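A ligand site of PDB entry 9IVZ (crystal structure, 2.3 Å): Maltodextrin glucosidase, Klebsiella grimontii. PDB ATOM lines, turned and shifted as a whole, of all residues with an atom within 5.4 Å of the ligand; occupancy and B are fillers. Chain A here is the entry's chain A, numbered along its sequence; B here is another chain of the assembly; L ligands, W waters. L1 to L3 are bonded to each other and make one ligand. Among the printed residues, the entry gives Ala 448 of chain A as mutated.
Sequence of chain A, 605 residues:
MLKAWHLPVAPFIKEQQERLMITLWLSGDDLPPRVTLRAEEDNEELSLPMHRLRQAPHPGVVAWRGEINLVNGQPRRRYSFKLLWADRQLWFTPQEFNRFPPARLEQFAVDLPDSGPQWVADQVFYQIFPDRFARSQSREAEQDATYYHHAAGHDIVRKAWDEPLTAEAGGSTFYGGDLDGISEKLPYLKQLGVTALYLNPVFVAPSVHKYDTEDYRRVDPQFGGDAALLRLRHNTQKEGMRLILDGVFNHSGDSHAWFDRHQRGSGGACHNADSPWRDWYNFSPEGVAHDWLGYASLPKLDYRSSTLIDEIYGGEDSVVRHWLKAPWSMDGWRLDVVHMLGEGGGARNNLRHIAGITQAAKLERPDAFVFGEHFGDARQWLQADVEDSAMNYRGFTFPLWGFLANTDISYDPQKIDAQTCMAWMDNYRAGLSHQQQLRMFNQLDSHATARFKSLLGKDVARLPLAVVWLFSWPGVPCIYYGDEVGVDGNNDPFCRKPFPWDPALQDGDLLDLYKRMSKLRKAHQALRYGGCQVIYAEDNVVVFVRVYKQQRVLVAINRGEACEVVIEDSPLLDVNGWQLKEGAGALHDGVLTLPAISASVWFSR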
ATOM      1  N   GLY A 170       1.233   7.790  -3.855  1.00  0.00           N
ATOM      2  CA  GLY A 170       0.159   8.566  -4.459  1.00  0.00           C
ATOM      3  C   GLY A 170      -1.223   8.288  -3.890  1.00  0.00           C
ATOM      4  O   GLY A 170      -2.097   9.150  -3.937  1.00  0.00           O
ATOM      5  N   GLY A 171      -1.440   7.103  -3.342  1.00  0.00           N
ATOM      6  CA  GLY A 171      -2.714   6.753  -2.763  1.00  0.00           C
ATOM      7  C   GLY A 171      -2.784   6.894  -1.273  1.00  0.00           C
ATOM      8  O   GLY A 171      -3.850   6.636  -0.690  1.00  0.00           O
ATOM      9  N   VAL A 208      -6.343   7.573   0.217  1.00  0.00           N
ATOM     10  CA  VAL A 208      -6.764   8.975   0.157  1.00  0.00           C
ATOM     11  C   VAL A 208      -7.910   9.149  -0.827  1.00  0.00           C
ATOM     12  O   VAL A 208      -8.759  10.029  -0.638  1.00  0.00           O
ATOM     13  CB  VAL A 208      -5.572   9.873  -0.206  1.00  0.00           C
ATOM     14  CG1 VAL A 208      -5.046   9.541  -1.615  1.00  0.00           C
ATOM     15  CG2 VAL A 208      -5.955  11.342  -0.115  1.00  0.00           C
ATOM     16  N   HIS A 209      -7.980   8.340  -1.882  1.00  0.00           N
ATOM     17  CA  HIS A 209      -9.057   8.467  -2.856  1.00  0.00           C
ATOM     18  C   HIS A 209     -10.305   7.703  -2.443  1.00  0.00           C
ATOM     19  O   HIS A 209     -11.417   8.091  -2.814  1.00  0.00           O
ATOM     20  CB  HIS A 209      -8.557   7.999  -4.216  1.00  0.00           C
ATOM     21  CG  HIS A 209      -7.969   6.623  -4.196  1.00  0.00           C
ATOM     22  ND1 HIS A 209      -8.747   5.485  -4.091  1.00  0.00           N
ATOM     23  CD2 HIS A 209      -6.688   6.207  -4.199  1.00  0.00           C
ATOM     24  CE1 HIS A 209      -7.960   4.430  -4.045  1.00  0.00           C
ATOM     25  NE2 HIS A 209      -6.704   4.832  -4.121  1.00  0.00           N
ATOM     26  N   TYR A 211     -11.576   4.703  -3.165  1.00  0.00           N
ATOM     27  CA  TYR A 211     -12.286   3.709  -3.978  1.00  0.00           C
ATOM     28  C   TYR A 211     -12.082   2.303  -3.438  1.00  0.00           C
ATOM     29  O   TYR A 211     -12.692   1.355  -3.946  1.00  0.00           O
ATOM     30  CB  TYR A 211     -11.852   3.792  -5.446  1.00  0.00           C
ATOM     31  CG  TYR A 211     -12.397   5.012  -6.155  1.00  0.00           C
ATOM     32  CD1 TYR A 211     -13.725   5.049  -6.590  1.00  0.00           C
ATOM     33  CD2 TYR A 211     -11.607   6.130  -6.368  1.00  0.00           C
ATOM     34  CE1 TYR A 211     -14.247   6.180  -7.231  1.00  0.00           C
ATOM     35  CE2 TYR A 211     -12.121   7.274  -6.985  1.00  0.00           C
ATOM     36  CZ  TYR A 211     -13.433   7.288  -7.413  1.00  0.00           C
ATOM     37  OH  TYR A 211     -13.919   8.434  -8.023  1.00  0.00           O
ATOM     38  N   VAL A 248     -19.320   3.174  -5.472  1.00  0.00           N
ATOM     39  CA  VAL A 248     -18.245   2.255  -5.860  1.00  0.00           C
ATOM     40  C   VAL A 248     -18.697   0.813  -5.628  1.00  0.00           C
ATOM     41  O   VAL A 248     -18.372   0.211  -4.611  1.00  0.00           O
ATOM     42  CB  VAL A 248     -16.952   2.566  -5.094  1.00  0.00           C
ATOM     43  CG1 VAL A 248     -15.746   1.869  -5.754  1.00  0.00           C
ATOM     44  CG2 VAL A 248     -16.737   4.083  -5.026  1.00  0.00           C
ATOM     45  N   HIS A 251     -16.545  -3.181  -7.023  1.00  0.00           N
ATOM     46  CA  HIS A 251     -15.502  -3.796  -6.233  1.00  0.00           C
ATOM     47  C   HIS A 251     -15.509  -3.140  -4.859  1.00  0.00           C
ATOM     48  O   HIS A 251     -15.932  -1.995  -4.720  1.00  0.00           O
ATOM     49  CB  HIS A 251     -14.143  -3.616  -6.912  1.00  0.00           C
ATOM     50  CG  HIS A 251     -13.725  -2.183  -6.989  1.00  0.00           C
ATOM     51  ND1 HIS A 251     -13.851  -1.422  -8.130  1.00  0.00           N
ATOM     52  CD2 HIS A 251     -13.233  -1.347  -6.039  1.00  0.00           C
ATOM     53  CE1 HIS A 251     -13.421  -0.197  -7.897  1.00  0.00           C
ATOM     54  NE2 HIS A 251     -13.047  -0.124  -6.628  1.00  0.00           N
ATOM     55  N   TRP A 292      -8.222  -8.359  -8.791  1.00  0.00           N
ATOM     56  CA  TRP A 292      -9.012  -7.771  -9.875  1.00  0.00           C
ATOM     57  C   TRP A 292      -8.092  -6.887 -10.701  1.00  0.00           C
ATOM     58  O   TRP A 292      -7.463  -5.971 -10.168  1.00  0.00           O
ATOM     59  CB  TRP A 292     -10.210  -6.967  -9.367  1.00  0.00           C
ATOM     60  CG  TRP A 292     -10.958  -6.343 -10.523  1.00  0.00           C
ATOM     61  CD1 TRP A 292     -11.484  -7.000 -11.607  1.00  0.00           C
ATOM     62  CD2 TRP A 292     -11.251  -4.952 -10.725  1.00  0.00           C
ATOM     63  NE1 TRP A 292     -12.074  -6.100 -12.473  1.00  0.00           N
ATOM     64  CE2 TRP A 292     -11.954  -4.845 -11.953  1.00  0.00           C
ATOM     65  CE3 TRP A 292     -11.003  -3.780  -9.993  1.00  0.00           C
ATOM     66  CZ2 TRP A 292     -12.397  -3.611 -12.449  1.00  0.00           C
ATOM     67  CZ3 TRP A 292     -11.441  -2.578 -10.490  1.00  0.00           C
ATOM     68  CH2 TRP A 292     -12.136  -2.498 -11.708  1.00  0.00           C
ATOM     69  N   LEU A 293      -8.052  -7.147 -12.001  1.00  0.00           N
ATOM     70  CA  LEU A 293      -7.062  -6.519 -12.879  1.00  0.00           C
ATOM     71  C   LEU A 293      -5.704  -6.625 -12.192  1.00  0.00           C
ATOM     72  O   LEU A 293      -5.275  -7.721 -11.833  1.00  0.00           O
ATOM     73  CB  LEU A 293      -7.429  -5.071 -13.200  1.00  0.00           C
ATOM     74  CG  LEU A 293      -8.776  -4.900 -13.939  1.00  0.00           C
ATOM     75  CD1 LEU A 293      -8.905  -3.519 -14.571  1.00  0.00           C
ATOM     76  CD2 LEU A 293      -9.040  -5.986 -14.970  1.00  0.00           C
ATOM     77  N   TYR A 295      -5.077  -5.324  -9.206  1.00  0.00           N
ATOM     78  CA  TYR A 295      -5.254  -4.801  -7.852  1.00  0.00           C
ATOM     79  C   TYR A 295      -5.552  -5.905  -6.861  1.00  0.00           C
ATOM     80  O   TYR A 295      -6.608  -6.552  -6.933  1.00  0.00           O
ATOM     81  CB  TYR A 295      -6.390  -3.775  -7.823  1.00  0.00           C
ATOM     82  CG  TYR A 295      -6.202  -2.629  -8.768  1.00  0.00           C
ATOM     83  CD1 TYR A 295      -5.278  -1.628  -8.483  1.00  0.00           C
ATOM     84  CD2 TYR A 295      -6.962  -2.535  -9.931  1.00  0.00           C
ATOM     85  CE1 TYR A 295      -5.104  -0.546  -9.335  1.00  0.00           C
ATOM     86  CE2 TYR A 295      -6.792  -1.459 -10.795  1.00  0.00           C
ATOM     87  CZ  TYR A 295      -5.856  -0.464 -10.495  1.00  0.00           C
ATOM     88  OH  TYR A 295      -5.671   0.613 -11.332  1.00  0.00           O
ATOM     89  N   SER A 297      -5.823  -4.649  -3.881  1.00  0.00           N
ATOM     90  CA  SER A 297      -6.593  -3.816  -2.958  1.00  0.00           C
ATOM     91  C   SER A 297      -8.069  -3.713  -3.321  1.00  0.00           C
ATOM     92  O   SER A 297      -8.863  -3.327  -2.459  1.00  0.00           O
ATOM     93  CB  SER A 297      -5.990  -2.413  -2.875  1.00  0.00           C
ATOM     94  OG  SER A 297      -5.928  -1.814  -4.151  1.00  0.00           O
ATOM     95  N   LEU A 298      -8.460  -4.042  -4.550  1.00  0.00           N
ATOM     96  CA  LEU A 298      -9.807  -3.764  -5.055  1.00  0.00           C
ATOM     97  C   LEU A 298     -10.505  -5.021  -5.564  1.00  0.00           C
ATOM     98  O   LEU A 298     -10.888  -5.090  -6.734  1.00  0.00           O
ATOM     99  CB  LEU A 298      -9.763  -2.707  -6.156  1.00  0.00           C
ATOM    100  CG  LEU A 298      -9.018  -1.392  -5.911  1.00  0.00           C
ATOM    101  CD1 LEU A 298      -8.865  -0.594  -7.174  1.00  0.00           C
ATOM    102  CD2 LEU A 298      -9.744  -0.572  -4.856  1.00  0.00           C
ATOM    103  N   ASP A 336     -19.124   4.389 -10.114  1.00  0.00           N
ATOM    104  CA  ASP A 336     -17.740   4.106 -10.476  1.00  0.00           C
ATOM    105  C   ASP A 336     -17.645   2.763 -11.192  1.00  0.00           C
ATOM    106  O   ASP A 336     -18.365   1.829 -10.838  1.00  0.00           O
ATOM    107  CB  ASP A 336     -16.871   4.095  -9.223  1.00  0.00           C
ATOM    108  CG  ASP A 336     -15.402   3.835  -9.526  1.00  0.00           C
ATOM    109  OD1 ASP A 336     -14.811   4.612 -10.294  1.00  0.00           O
ATOM    110  OD2 ASP A 336     -14.837   2.863  -8.992  1.00  0.00           O
ATOM    111  N   VAL A 337     -16.760   2.678 -12.189  1.00  0.00           N
ATOM    112  CA  VAL A 337     -16.561   1.474 -13.013  1.00  0.00           C
ATOM    113  C   VAL A 337     -17.901   0.887 -13.410  1.00  0.00           C
ATOM    114  O   VAL A 337     -18.161  -0.300 -13.183  1.00  0.00           O
ATOM    115  CB  VAL A 337     -15.693   0.426 -12.268  1.00  0.00           C
ATOM    116  CG1 VAL A 337     -15.177  -0.634 -13.247  1.00  0.00           C
ATOM    117  CG2 VAL A 337     -14.538   1.071 -11.540  1.00  0.00           C
ATOM    118  N   HIS A 339     -19.207   0.173 -16.231  1.00  0.00           N
ATOM    119  CA  HIS A 339     -19.202  -0.701 -17.393  1.00  0.00           C
ATOM    120  C   HIS A 339     -18.643  -2.096 -17.109  1.00  0.00           C
ATOM    121  O   HIS A 339     -18.780  -2.984 -17.957  1.00  0.00           O
ATOM    122  CB  HIS A 339     -18.390  -0.038 -18.502  1.00  0.00           C
ATOM    123  CG  HIS A 339     -16.935   0.140 -18.155  1.00  0.00           C
ATOM    124  ND1 HIS A 339     -16.517   0.705 -16.968  1.00  0.00           N
ATOM    125  CD2 HIS A 339     -15.809  -0.196 -18.836  1.00  0.00           C
ATOM    126  CE1 HIS A 339     -15.197   0.721 -16.941  1.00  0.00           C
ATOM    127  NE2 HIS A 339     -14.745   0.181 -18.054  1.00  0.00           N
ATOM    128  N   MET A 340     -18.001  -2.322 -15.966  1.00  0.00           N
ATOM    129  CA  MET A 340     -17.383  -3.612 -15.704  1.00  0.00           C
ATOM    130  C   MET A 340     -18.066  -4.396 -14.593  1.00  0.00           C
ATOM    131  O   MET A 340     -17.814  -5.597 -14.463  1.00  0.00           O
ATOM    132  CB  MET A 340     -15.903  -3.446 -15.367  1.00  0.00           C
ATOM    133  CG  MET A 340     -15.127  -2.713 -16.451  1.00  0.00           C
ATOM    134  SD  MET A 340     -13.361  -2.574 -16.133  1.00  0.00           S
ATOM    135  CE  MET A 340     -12.829  -4.241 -16.526  1.00  0.00           C
ATOM    136  N   GLU A 373     -19.502   6.431 -14.889  1.00  0.00           N
ATOM    137  CA  GLU A 373     -18.251   6.861 -15.500  1.00  0.00           C
ATOM    138  C   GLU A 373     -17.978   5.991 -16.722  1.00  0.00           C
ATOM    139  O   GLU A 373     -17.691   4.797 -16.591  1.00  0.00           O
ATOM    140  CB  GLU A 373     -17.102   6.763 -14.505  1.00  0.00           C
ATOM    141  CG  GLU A 373     -15.757   7.043 -15.137  1.00  0.00           C
ATOM    142  CD  GLU A 373     -14.579   6.676 -14.233  1.00  0.00           C
ATOM    143  OE1 GLU A 373     -14.387   5.462 -13.931  1.00  0.00           O
ATOM    144  OE2 GLU A 373     -13.851   7.625 -13.829  1.00  0.00           O
ATOM    145  N   PHE A 375     -15.427   6.086 -19.679  1.00  0.00           N
ATOM    146  CA  PHE A 375     -14.346   6.447 -20.603  1.00  0.00           C
ATOM    147  C   PHE A 375     -14.660   5.990 -22.015  1.00  0.00           C
ATOM    148  O   PHE A 375     -14.201   6.603 -22.989  1.00  0.00           O
ATOM    149  CB  PHE A 375     -13.024   5.854 -20.125  1.00  0.00           C
ATOM    150  CG  PHE A 375     -12.308   6.705 -19.105  1.00  0.00           C
ATOM    151  CD1 PHE A 375     -12.828   6.848 -17.818  1.00  0.00           C
ATOM    152  CD2 PHE A 375     -11.156   7.381 -19.436  1.00  0.00           C
ATOM    153  CE1 PHE A 375     -12.187   7.648 -16.864  1.00  0.00           C
ATOM    154  CE2 PHE A 375     -10.499   8.188 -18.492  1.00  0.00           C
ATOM    155  CZ  PHE A 375     -11.025   8.319 -17.205  1.00  0.00           C
ATOM    156  N   HIS A 447     -10.497  13.440 -11.790  1.00  0.00           N
ATOM    157  CA  HIS A 447      -9.516  12.790 -10.940  1.00  0.00           C
ATOM    158  C   HIS A 447      -8.800  11.631 -11.622  1.00  0.00           C
ATOM    159  O   HIS A 447      -7.824  11.117 -11.073  1.00  0.00           O
ATOM    160  CB  HIS A 447     -10.196  12.276  -9.683  1.00  0.00           C
ATOM    161  CG  HIS A 447     -11.202  11.219  -9.964  1.00  0.00           C
ATOM    162  ND1 HIS A 447     -12.379  11.484 -10.630  1.00  0.00           N
ATOM    163  CD2 HIS A 447     -11.194   9.880  -9.722  1.00  0.00           C
ATOM    164  CE1 HIS A 447     -13.074  10.355 -10.769  1.00  0.00           C
ATOM    165  NE2 HIS A 447     -12.372   9.375 -10.226  1.00  0.00           N
ATOM    166  N   ALA A 448      -9.295  11.185 -12.786  1.00  0.00           N
ATOM    167  CA  ALA A 448      -8.762  10.040 -13.507  1.00  0.00           C
ATOM    168  C   ALA A 448      -8.098  10.429 -14.821  1.00  0.00           C
ATOM    169  O   ALA A 448      -7.752   9.547 -15.619  1.00  0.00           O
ATOM    170  CB  ALA A 448      -9.866   9.012 -13.754  1.00  0.00           C
ATOM    171  N   ASP A 492      -3.115  11.392 -12.638  1.00  0.00           N
ATOM    172  CA  ASP A 492      -3.106  10.683 -11.364  1.00  0.00           C
ATOM    173  C   ASP A 492      -1.716  10.123 -11.069  1.00  0.00           C
ATOM    174  O   ASP A 492      -1.233   9.248 -11.800  1.00  0.00           O
ATOM    175  CB  ASP A 492      -4.160   9.577 -11.442  1.00  0.00           C
ATOM    176  CG  ASP A 492      -4.325   8.831 -10.151  1.00  0.00           C
ATOM    177  OD1 ASP A 492      -3.859   9.321  -9.106  1.00  0.00           O
ATOM    178  OD2 ASP A 492      -4.938   7.734 -10.185  1.00  0.00           O
ATOM    179  N   PRO A 493      -1.056  10.571  -9.992  1.00  0.00           N
ATOM    180  CA  PRO A 493      -1.541  11.406  -8.881  1.00  0.00           C
ATOM    181  C   PRO A 493      -1.570  12.934  -9.093  1.00  0.00           C
ATOM    182  O   PRO A 493      -2.196  13.617  -8.281  1.00  0.00           O
ATOM    183  CB  PRO A 493      -0.558  11.057  -7.769  1.00  0.00           C
ATOM    184  CG  PRO A 493       0.723  10.861  -8.493  1.00  0.00           C
ATOM    185  CD  PRO A 493       0.327  10.123  -9.758  1.00  0.00           C
ATOM    186  N   ARG A 496      -4.566  15.794  -8.851  1.00  0.00           N
ATOM    187  CA  ARG A 496      -5.263  15.986  -7.581  1.00  0.00           C
ATOM    188  C   ARG A 496      -4.496  16.947  -6.680  1.00  0.00           C
ATOM    189  O   ARG A 496      -4.331  16.696  -5.481  1.00  0.00           O
ATOM    190  CB  ARG A 496      -5.478  14.637  -6.897  1.00  0.00           C
ATOM    191  CG  ARG A 496      -6.191  13.637  -7.788  1.00  0.00           C
ATOM    192  CD  ARG A 496      -5.983  12.206  -7.352  1.00  0.00           C
ATOM    193  NE  ARG A 496      -6.577  11.323  -8.345  1.00  0.00           N
ATOM    194  CZ  ARG A 496      -6.881  10.047  -8.143  1.00  0.00           C
ATOM    195  NH1 ARG A 496      -6.617   9.448  -6.986  1.00  0.00           N
ATOM    196  NH2 ARG A 496      -7.472   9.364  -9.121  1.00  0.00           N
ATOM    197  N   GLU B  44     -14.010  -2.753 -21.024  1.00  0.00           N
ATOM    198  CA  GLU B  44     -12.924  -1.786 -20.888  1.00  0.00           C
ATOM    199  C   GLU B  44     -12.111  -1.744 -22.178  1.00  0.00           C
ATOM    200  O   GLU B  44     -11.757  -2.786 -22.737  1.00  0.00           O
ATOM    201  CB  GLU B  44     -12.030  -2.134 -19.708  1.00  0.00           C
ATOM    202  CG  GLU B  44     -10.751  -1.308 -19.613  1.00  0.00           C
ATOM    203  CD  GLU B  44     -10.985   0.083 -19.049  1.00  0.00           C
ATOM    204  OE1 GLU B  44     -12.122   0.582 -19.139  1.00  0.00           O
ATOM    205  OE2 GLU B  44     -10.019   0.675 -18.521  1.00  0.00           O
HETATM  206  C1  LIG L   1     -10.375   3.873 -17.188  1.00  0.00           C
HETATM  207  C2  LIG L   1     -11.425   2.955 -16.575  1.00  0.00           C
HETATM  208  C3  LIG L   1     -11.937   3.444 -15.238  1.00  0.00           C
HETATM  209  C4  LIG L   1     -10.991   4.363 -14.462  1.00  0.00           C
HETATM  210  C5  LIG L   1      -9.613   4.713 -15.082  1.00  0.00           C
HETATM  211  C6  LIG L   1      -8.498   4.809 -14.098  1.00  0.00           C
HETATM  212  O1  LIG L   1      -9.958   3.387 -18.464  1.00  0.00           O
HETATM  213  O2  LIG L   1     -12.497   2.832 -17.510  1.00  0.00           O
HETATM  214  O3  LIG L   1     -12.481   2.336 -14.478  1.00  0.00           O
HETATM  215  O4  LIG L   1     -10.994   4.403 -12.994  1.00  0.00           O
HETATM  216  O5  LIG L   1      -9.222   3.913 -16.278  1.00  0.00           O
HETATM  217  O6  LIG L   1      -7.601   3.767 -14.289  1.00  0.00           O
HETATM  218  C1  LG2 L   2     -10.956   3.342 -12.088  1.00  0.00           C
HETATM  219  C2  LG2 L   2     -11.451   3.963 -10.796  1.00  0.00           C
HETATM  220  C3  LG2 L   2     -11.122   3.249  -9.547  1.00  0.00           C
HETATM  221  C4  LG2 L   2      -9.733   2.721  -9.489  1.00  0.00           C
HETATM  222  C5  LG2 L   2      -9.284   2.059 -10.787  1.00  0.00           C
HETATM  223  C6  LG2 L   2      -9.905   0.664 -11.024  1.00  0.00           C
HETATM  224  O1  LG2 L   2     -10.916   5.342 -10.656  1.00  0.00           O
HETATM  225  O2  LG2 L   2     -12.115   2.192  -9.341  1.00  0.00           O
HETATM  226  O3  LG2 L   2      -8.782   3.857  -9.230  1.00  0.00           O
HETATM  227  O4  LG2 L   2      -9.556   2.871 -11.979  1.00  0.00           O
HETATM  228  O5  LG2 L   2      -9.399   0.170 -12.266  1.00  0.00           O
HETATM  229  O1  LG3 L   3      -7.830   3.230  -7.106  1.00  0.00           O
HETATM  230  C1  LG3 L   3      -7.886   5.571  -7.796  1.00  0.00           C
HETATM  231  C2  LG3 L   3      -6.489   5.524  -8.335  1.00  0.00           C
HETATM  232  C3  LG3 L   3      -3.010   5.872  -6.287  1.00  0.00           C
HETATM  233  C4  LG3 L   3       0.213   3.373  -7.741  1.00  0.00           C
HETATM  234  C5  LG3 L   3      -1.061   4.253  -7.737  1.00  0.00           C
HETATM  235  C6  LG3 L   3      -2.368   3.560  -7.070  1.00  0.00           C
HETATM  236  C7  LG3 L   3      -3.535   4.343  -6.815  1.00  0.00           C
HETATM  237  C8  LG3 L   3      -5.738   4.206  -8.288  1.00  0.00           C
HETATM  238  C9  LG3 L   3      -6.512   2.932  -7.751  1.00  0.00           C
HETATM  239  C10 LG3 L   3      -5.800   1.937  -6.893  1.00  0.00           C
HETATM  240  C11 LG3 L   3      -8.609   4.223  -7.860  1.00  0.00           C
HETATM  241  C12 LG3 L   3      -2.402   6.479  -7.272  1.00  0.00           C
HETATM  242  C13 LG3 L   3      -0.911   5.682  -7.597  1.00  0.00           C
HETATM  243  N1  LG3 L   3      -4.226   4.429  -8.087  1.00  0.00           N
HETATM  244  O2  LG3 L   3       1.188   3.915  -8.638  1.00  0.00           O
HETATM  245  O3  LG3 L   3      -8.606   6.483  -8.611  1.00  0.00           O
HETATM  246  O4  LG3 L   3      -5.711   6.644  -7.817  1.00  0.00           O
HETATM  247  O5  LG3 L   3      -4.159   6.607  -5.802  1.00  0.00           O
HETATM  248  O6  LG3 L   3      -2.103   7.872  -6.998  1.00  0.00           O
HETATM  249  O7  LG3 L   3      -0.371   6.243  -8.743  1.00  0.00           O
HETATM  250  O   HOH W   1     -13.218   6.595 -10.935  1.00  0.00           O
HETATM  251  O   HOH W   2      -6.982   6.829 -12.011  1.00  0.00           O
HETATM  252  O   HOH W   3       3.414   4.196 -10.325  1.00  0.00           O
HETATM  253  O   HOH W   4     -15.155   3.958 -17.640  1.00  0.00           O
HETATM  254  O   HOH W   5     -11.374   0.041 -14.263  1.00  0.00           O
HETATM  255  O   HOH W   6      -3.775   2.854 -10.191  1.00  0.00           O
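The side-chain sulfur of Met 340 sits close to a ring nitrogen (NE2) of His 339 (3.6 Å).
N of Tyr 211 is in hydrogen-bond range of ND1 of His 209 (3.1 Å).
NH2 of Arg 496 lies within hydrogen-bond range of O of His 447 (2.6 Å).
The side-chain hydroxyl (OH) of Tyr 211 sits at hydrogen-bond distance from a ring nitrogen (NE2) of His 447 (2.9 Å).
A ring nitrogen (NE2) of His 251 sits at hydrogen-bond distance from the backbone carbonyl oxygen of Tyr 211, at 3.1 Å.
NE2 of His 339 is in hydrogen-bond range of OE1 of Glu 44 of chain B, at 2.9 Å.
O of Gly 171 is in hydrogen-bond range of N of Val 208.
The guanidinium group of Arg 496 is in salt-bridge range of the side-chain carboxylate of Asp 492 (3.2 Å).
Water W5 bridges an oxygen (O3) of LIG L1 (2.6 Å) and the side-chain sulfur of Met 340 (3.8 Å).
Water W1 lies within hydrogen-bond range of OD1 of Asp 336, O1 of LG2 L2, NE2 of His 447 and OE2 of Glu 373.
Water W6 lies within hydrogen-bond range of a nitrogen (N1) of LG3 L3 (2.7 Å) and the side-chain hydroxyl (OH) of Tyr 295 (3.1 Å).
Water W4 lies within hydrogen-bond range of the backbone carbonyl oxygen of Glu 373 (2.9 Å), an oxygen (O2) of LIG L1 (2.9 Å) and the backbone NH of Phe 375 (3.0 Å).
The backbone carbonyl oxygen (O) of Gly 170 sits close to an oxygen (O6) of LG3 L3, at 3.3 Å.
An oxygen (O1) of LIG L1 sits at hydrogen-bond distance from the side-chain carboxylate (OE2) of Glu 44 of chain B (2.7 Å).
A nitrogen (N1) of LG3 L3 is in salt-bridge range of the side-chain carboxylate (OD2) of Asp 492, at 3.98 Å.
OD2 of Asp 336 lies within hydrogen-bond range of O2 of LG2 L2, at 2.8 Å.
O4 of LG3 L3 sits at hydrogen-bond distance from NH1 of Arg 496 (3.1 Å).
Residues that only touch the ligand: His 209 (3.0 Å), His 251 (3.1 Å), Gly 171 (3.4 Å), Tyr 295 (3.4 Å), Glu 373 (3.4 Å), Val 337 (3.5 Å), His 339 (3.5 Å), Pro 493 (3.6 Å), Trp 292 (3.6 Å), Tyr 211 (3.8 Å), Phe 375 (3.9 Å) and Leu 298 (3.96 Å).
Hydrophobic or aromatic side chains within 4 Å of the ligand: His 209, Tyr 211, His 251, Trp 292, Tyr 295, Leu 298, Val 337, His 339, Phe 375 and Pro 493.
Within 4 Å of the ligand: Gly 170, Gly 171, His 209, Tyr 211, His 251, Trp 292, Tyr 295, Leu 298, Asp 336, Val 337, His 339, Glu 373, Phe 375, Asp 492, Pro 493, Arg 496 and Glu 44 of chain B.
The nearest printed residue that does not touch the ligand is His 447 (4.3 Å).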
